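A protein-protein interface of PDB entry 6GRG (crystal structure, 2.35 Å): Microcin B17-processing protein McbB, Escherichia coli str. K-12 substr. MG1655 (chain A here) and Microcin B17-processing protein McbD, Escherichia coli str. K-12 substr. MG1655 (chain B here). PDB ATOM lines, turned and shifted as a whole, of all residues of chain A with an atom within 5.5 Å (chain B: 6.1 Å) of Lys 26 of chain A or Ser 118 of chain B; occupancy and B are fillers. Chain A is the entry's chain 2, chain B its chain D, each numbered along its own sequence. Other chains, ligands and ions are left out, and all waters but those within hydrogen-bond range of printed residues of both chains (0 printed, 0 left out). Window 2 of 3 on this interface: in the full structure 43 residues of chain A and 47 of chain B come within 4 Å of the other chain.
The guanidinium group (NH1) of Arg 23 of chain A is in hydrogen-bond range of the backbone carbonyl oxygen (O) of Leu 116 of chain B (2.6 Å).
The backbone NH (N) of Leu 28 of chain A sits at hydrogen-bond distance from the backbone carbonyl oxygen (O) of Ile 21 of chain A (2.8 Å).
OD1 of Asn 115 of chain B is in hydrogen-bond range of N of Phe 117 of chain B, 2.9 Å away.
N of Ser 118 of chain B lies within hydrogen-bond range of OD1 of Asn 115 of chain B, 2.9 Å away.
OG of Ser 118 of chain B sits close to N of Glu 120 of chain B (3.2 Å).
Among the printed residues, merely in contact across the chains: Ile 21 of chain A with Leu 119 of chain B (3.3 Å), Arg 23 of chain A with Phe 117 of chain B (3.7 Å), Arg 23 of chain A with Leu 119 of chain B (3.9 Å), Lys 26 of chain A with Ser 118 of chain B (3.6 Å), Lys 26 of chain A with Leu 119 of chain B (3.9 Å) and Leu 28 of chain A with Leu 119 of chain B (3.9 Å).
Of the printed residues of chain B, Leu 28 of chain A touches Leu 119.
Printed residues of chain A within 4 Å of Leu 116 of chain B: Arg 23 (2.6 Å).
Of the printed residues of chain A, Phe 117 of chain B touches Arg 23.
Of chain A, only Lys 26 comes within 4 Å of Ser 118 of chain B.
Of the printed residues of chain A, Leu 119 of chain B touches Ile 21, Arg 23, Lys 26 and Leu 28.
The nearest printed residue of chain B that does not touch Lys 26 of chain A is Phe 117 of chain B (5.9 Å).
The nearest printed residue of chain A that does not touch Ser 118 of chain B is Arg 23 of chain A (5.5 Å).
Of the 9 printed residues of chain A, 4 touch a printed residue of chain B.
Printed residues of chain A that touch a printed residue of chain B: Ile 21, Arg 23, Lys 26 and Leu 28.
Hydrophobic or aromatic side chains of chain A within 4 Å of the printed part of chain B: Leu 28.
Hydrophobic or aromatic side chains of chain B within 4 Å of the printed part of chain A: Leu 116 and Leu 119.
Among the printed residues, 7 pairs touch across the chains.
Among the printed residues, no Asp or Glu carboxylate lies within 4 Å of a Lys or Arg side-chain nitrogen of the other chain.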
ATOM      1  N   ILE A  21     -15.909   1.067 -24.373  1.00  0.00           N
ATOM      2  CA  ILE A  21     -16.495   2.305 -23.853  1.00  0.00           C
ATOM      3  C   ILE A  21     -17.256   2.996 -24.998  1.00  0.00           C
ATOM      4  O   ILE A  21     -16.746   3.082 -26.126  1.00  0.00           O
ATOM      5  CB  ILE A  21     -15.395   3.195 -23.225  1.00  0.00           C
ATOM      6  CG1 ILE A  21     -15.955   4.518 -22.689  1.00  0.00           C
ATOM      7  CG2 ILE A  21     -14.247   3.424 -24.199  1.00  0.00           C
ATOM      8  CD1 ILE A  21     -15.204   5.069 -21.480  1.00  0.00           C
ATOM      9  N   SER A  22     -18.477   3.460 -24.702  1.00  0.00           N
ATOM     10  CA  SER A  22     -19.402   4.033 -25.702  1.00  0.00           C
ATOM     11  C   SER A  22     -19.921   5.401 -25.248  1.00  0.00           C
ATOM     12  O   SER A  22     -20.136   5.635 -24.078  1.00  0.00           O
ATOM     13  CB  SER A  22     -20.556   3.106 -25.972  1.00  0.00           C
ATOM     14  OG  SER A  22     -20.104   1.868 -26.485  1.00  0.00           O
ATOM     15  N   ARG A  23     -20.146   6.286 -26.218  1.00  0.00           N
ATOM     16  CA  ARG A  23     -20.515   7.698 -26.024  1.00  0.00           C
ATOM     17  C   ARG A  23     -20.825   8.238 -27.428  1.00  0.00           C
ATOM     18  O   ARG A  23     -20.138   7.860 -28.391  1.00  0.00           O
ATOM     19  CB  ARG A  23     -19.372   8.463 -25.342  1.00  0.00           C
ATOM     20  CG  ARG A  23     -19.766   9.274 -24.115  1.00  0.00           C
ATOM     21  CD  ARG A  23     -18.562   9.530 -23.214  1.00  0.00           C
ATOM     22  NE  ARG A  23     -18.439   8.542 -22.142  1.00  0.00           N
ATOM     23  CZ  ARG A  23     -17.446   8.470 -21.255  1.00  0.00           C
ATOM     24  NH1 ARG A  23     -16.395   9.265 -21.362  1.00  0.00           N
ATOM     25  NH2 ARG A  23     -17.505   7.594 -20.263  1.00  0.00           N
ATOM     26  N   ASN A  24     -21.868   9.071 -27.564  1.00  0.00           N
ATOM     27  CA  ASN A  24     -22.477   9.298 -28.883  1.00  0.00           C
ATOM     28  C   ASN A  24     -22.746   7.898 -29.472  1.00  0.00           C
ATOM     29  O   ASN A  24     -23.046   6.957 -28.713  1.00  0.00           O
ATOM     30  CB  ASN A  24     -21.610  10.214 -29.763  1.00  0.00           C
ATOM     31  N   THR A  25     -22.598   7.745 -30.796  1.00  0.00           N
ATOM     32  CA  THR A  25     -22.564   6.427 -31.444  1.00  0.00           C
ATOM     33  C   THR A  25     -21.128   5.892 -31.507  1.00  0.00           C
ATOM     34  O   THR A  25     -20.843   4.987 -32.311  1.00  0.00           O
ATOM     35  CB  THR A  25     -23.134   6.479 -32.866  1.00  0.00           C
ATOM     36  OG1 THR A  25     -22.279   7.303 -33.666  1.00  0.00           O
ATOM     37  CG2 THR A  25     -24.559   6.990 -32.897  1.00  0.00           C
ATOM     38  N   LYS A  26     -20.235   6.448 -30.675  1.00  0.00           N
ATOM     39  CA  LYS A  26     -18.809   6.111 -30.704  1.00  0.00           C
ATOM     40  C   LYS A  26     -18.540   4.938 -29.747  1.00  0.00           C
ATOM     41  O   LYS A  26     -19.235   4.783 -28.754  1.00  0.00           O
ATOM     42  CB  LYS A  26     -17.945   7.326 -30.336  1.00  0.00           C
ATOM     43  CG  LYS A  26     -17.893   8.444 -31.369  1.00  0.00           C
ATOM     44  CD  LYS A  26     -17.256   8.036 -32.694  1.00  0.00           C
ATOM     45  CE  LYS A  26     -16.114   8.934 -33.126  1.00  0.00           C
ATOM     46  NZ  LYS A  26     -15.942   8.902 -34.597  1.00  0.00           N
ATOM     47  N   THR A  27     -17.517   4.138 -30.069  1.00  0.00           N
ATOM     48  CA  THR A  27     -17.118   2.985 -29.277  1.00  0.00           C
ATOM     49  C   THR A  27     -15.605   2.781 -29.382  1.00  0.00           C
ATOM     50  O   THR A  27     -15.047   2.783 -30.454  1.00  0.00           O
ATOM     51  CB  THR A  27     -17.812   1.692 -29.732  1.00  0.00           C
ATOM     52  OG1 THR A  27     -19.226   1.855 -29.615  1.00  0.00           O
ATOM     53  CG2 THR A  27     -17.389   0.487 -28.925  1.00  0.00           C
ATOM     54  N   LEU A  28     -14.965   2.547 -28.241  1.00  0.00           N
ATOM     55  CA  LEU A  28     -13.542   2.347 -28.197  1.00  0.00           C
ATOM     56  C   LEU A  28     -13.265   1.030 -27.440  1.00  0.00           C
ATOM     57  O   LEU A  28     -13.688   0.832 -26.277  1.00  0.00           O
ATOM     58  CB  LEU A  28     -12.908   3.597 -27.559  1.00  0.00           C
ATOM     59  CG  LEU A  28     -11.412   3.546 -27.229  1.00  0.00           C
ATOM     60  CD1 LEU A  28     -10.560   3.355 -28.481  1.00  0.00           C
ATOM     61  CD2 LEU A  28     -10.979   4.803 -26.482  1.00  0.00           C
ATOM     62  N   ILE A  38     -14.133   1.370 -32.963  1.00  0.00           N
ATOM     63  CA  ILE A  38     -15.060   0.407 -33.495  1.00  0.00           C
ATOM     64  C   ILE A  38     -16.218   1.171 -34.139  1.00  0.00           C
ATOM     65  O   ILE A  38     -17.059   1.746 -33.441  1.00  0.00           O
ATOM     66  CB  ILE A  38     -15.539  -0.545 -32.377  1.00  0.00           C
ATOM     67  CG1 ILE A  38     -14.363  -1.113 -31.574  1.00  0.00           C
ATOM     68  CG2 ILE A  38     -16.416  -1.644 -32.951  1.00  0.00           C
ATOM     69  CD1 ILE A  38     -13.430  -2.004 -32.376  1.00  0.00           C
ATOM     70  N   ASN B 115     -10.279  11.518 -25.758  1.00  0.00           N
ATOM     71  CA  ASN B 115     -11.144  12.626 -25.414  1.00  0.00           C
ATOM     72  C   ASN B 115     -12.355  12.074 -24.636  1.00  0.00           C
ATOM     73  O   ASN B 115     -13.007  11.112 -25.084  1.00  0.00           O
ATOM     74  CB  ASN B 115     -11.500  13.435 -26.659  1.00  0.00           C
ATOM     75  CG  ASN B 115     -12.450  14.568 -26.359  1.00  0.00           C
ATOM     76  OD1 ASN B 115     -13.659  14.368 -26.264  1.00  0.00           O
ATOM     77  ND2 ASN B 115     -11.903  15.758 -26.206  1.00  0.00           N
ATOM     78  N   LEU B 116     -12.646  12.695 -23.481  1.00  0.00           N
ATOM     79  CA  LEU B 116     -13.715  12.251 -22.535  1.00  0.00           C
ATOM     80  C   LEU B 116     -15.067  12.147 -23.253  1.00  0.00           C
ATOM     81  O   LEU B 116     -15.893  11.289 -22.918  1.00  0.00           O
ATOM     82  CB  LEU B 116     -13.806  13.224 -21.352  1.00  0.00           C
ATOM     83  CG  LEU B 116     -14.774  12.833 -20.233  1.00  0.00           C
ATOM     84  CD1 LEU B 116     -14.286  11.601 -19.479  1.00  0.00           C
ATOM     85  CD2 LEU B 116     -14.987  13.971 -19.247  1.00  0.00           C
ATOM     86  N   PHE B 117     -15.286  13.019 -24.247  1.00  0.00           N
ATOM     87  CA  PHE B 117     -16.593  13.195 -24.873  1.00  0.00           C
ATOM     88  C   PHE B 117     -16.717  12.337 -26.145  1.00  0.00           C
ATOM     89  O   PHE B 117     -17.695  11.572 -26.271  1.00  0.00           O
ATOM     90  CB  PHE B 117     -16.828  14.688 -25.095  1.00  0.00           C
ATOM     91  CG  PHE B 117     -16.660  15.509 -23.842  1.00  0.00           C
ATOM     92  CD1 PHE B 117     -17.525  15.351 -22.772  1.00  0.00           C
ATOM     93  CD2 PHE B 117     -15.615  16.412 -23.717  1.00  0.00           C
ATOM     94  CE1 PHE B 117     -17.360  16.096 -21.613  1.00  0.00           C
ATOM     95  CE2 PHE B 117     -15.446  17.156 -22.556  1.00  0.00           C
ATOM     96  CZ  PHE B 117     -16.326  17.003 -21.508  1.00  0.00           C
ATOM     97  N   SER B 118     -15.728  12.443 -27.049  1.00  0.00           N
ATOM     98  CA  SER B 118     -15.750  11.855 -28.403  1.00  0.00           C
ATOM     99  C   SER B 118     -15.027  10.498 -28.469  1.00  0.00           C
ATOM    100  O   SER B 118     -15.087   9.815 -29.496  1.00  0.00           O
ATOM    101  CB  SER B 118     -15.107  12.803 -29.373  1.00  0.00           C
ATOM    102  OG  SER B 118     -13.696  12.848 -29.164  1.00  0.00           O
ATOM    103  N   LEU B 119     -14.260  10.166 -27.422  1.00  0.00           N
ATOM    104  CA  LEU B 119     -13.444   8.948 -27.354  1.00  0.00           C
ATOM    105  C   LEU B 119     -12.333   8.978 -28.403  1.00  0.00           C
ATOM    106  O   LEU B 119     -11.688   7.964 -28.638  1.00  0.00           O
ATOM    107  CB  LEU B 119     -14.327   7.710 -27.536  1.00  0.00           C
ATOM    108  CG  LEU B 119     -15.473   7.579 -26.531  1.00  0.00           C
ATOM    109  CD1 LEU B 119     -16.239   6.278 -26.742  1.00  0.00           C
ATOM    110  CD2 LEU B 119     -14.951   7.682 -25.100  1.00  0.00           C
ATOM    111  N   GLU B 120     -12.085  10.145 -28.994  1.00  0.00           N
ATOM    112  CA  GLU B 120     -11.058  10.256 -30.010  1.00  0.00           C
ATOM    113  C   GLU B 120      -9.699   9.984 -29.349  1.00  0.00           C
ATOM    114  O   GLU B 120      -9.384  10.540 -28.304  1.00  0.00           O
ATOM    115  CB  GLU B 120     -11.101  11.618 -30.707  1.00  0.00           C
ATOM    116  CG  GLU B 120      -9.951  11.799 -31.692  1.00  0.00           C
ATOM    117  CD  GLU B 120      -9.867  13.121 -32.442  1.00  0.00           C
ATOM    118  OE1 GLU B 120     -10.438  14.130 -31.964  1.00  0.00           O
ATOM    119  OE2 GLU B 120      -9.224  13.130 -33.509  1.00  0.00           O
ATOM    120  N   GLN B 332     -18.789  19.537 -21.000  1.00  0.00           N
ATOM    121  CA  GLN B 332     -18.492  19.804 -22.414  1.00  0.00           C
ATOM    122  C   GLN B 332     -18.924  21.231 -22.768  1.00  0.00           C
ATOM    123  O   GLN B 332     -18.267  21.878 -23.571  1.00  0.00           O
ATOM    124  CB  GLN B 332     -19.141  18.788 -23.362  1.00  0.00           C
ATOM    125  CG  GLN B 332     -18.756  19.001 -24.830  1.00  0.00           C
ATOM    126  CD  GLN B 332     -19.039  17.826 -25.743  1.00  0.00           C
ATOM    127  OE1 GLN B 332     -19.927  17.009 -25.502  1.00  0.00           O
ATOM    128  NE2 GLN B 332     -18.279  17.729 -26.822  1.00  0.00           N
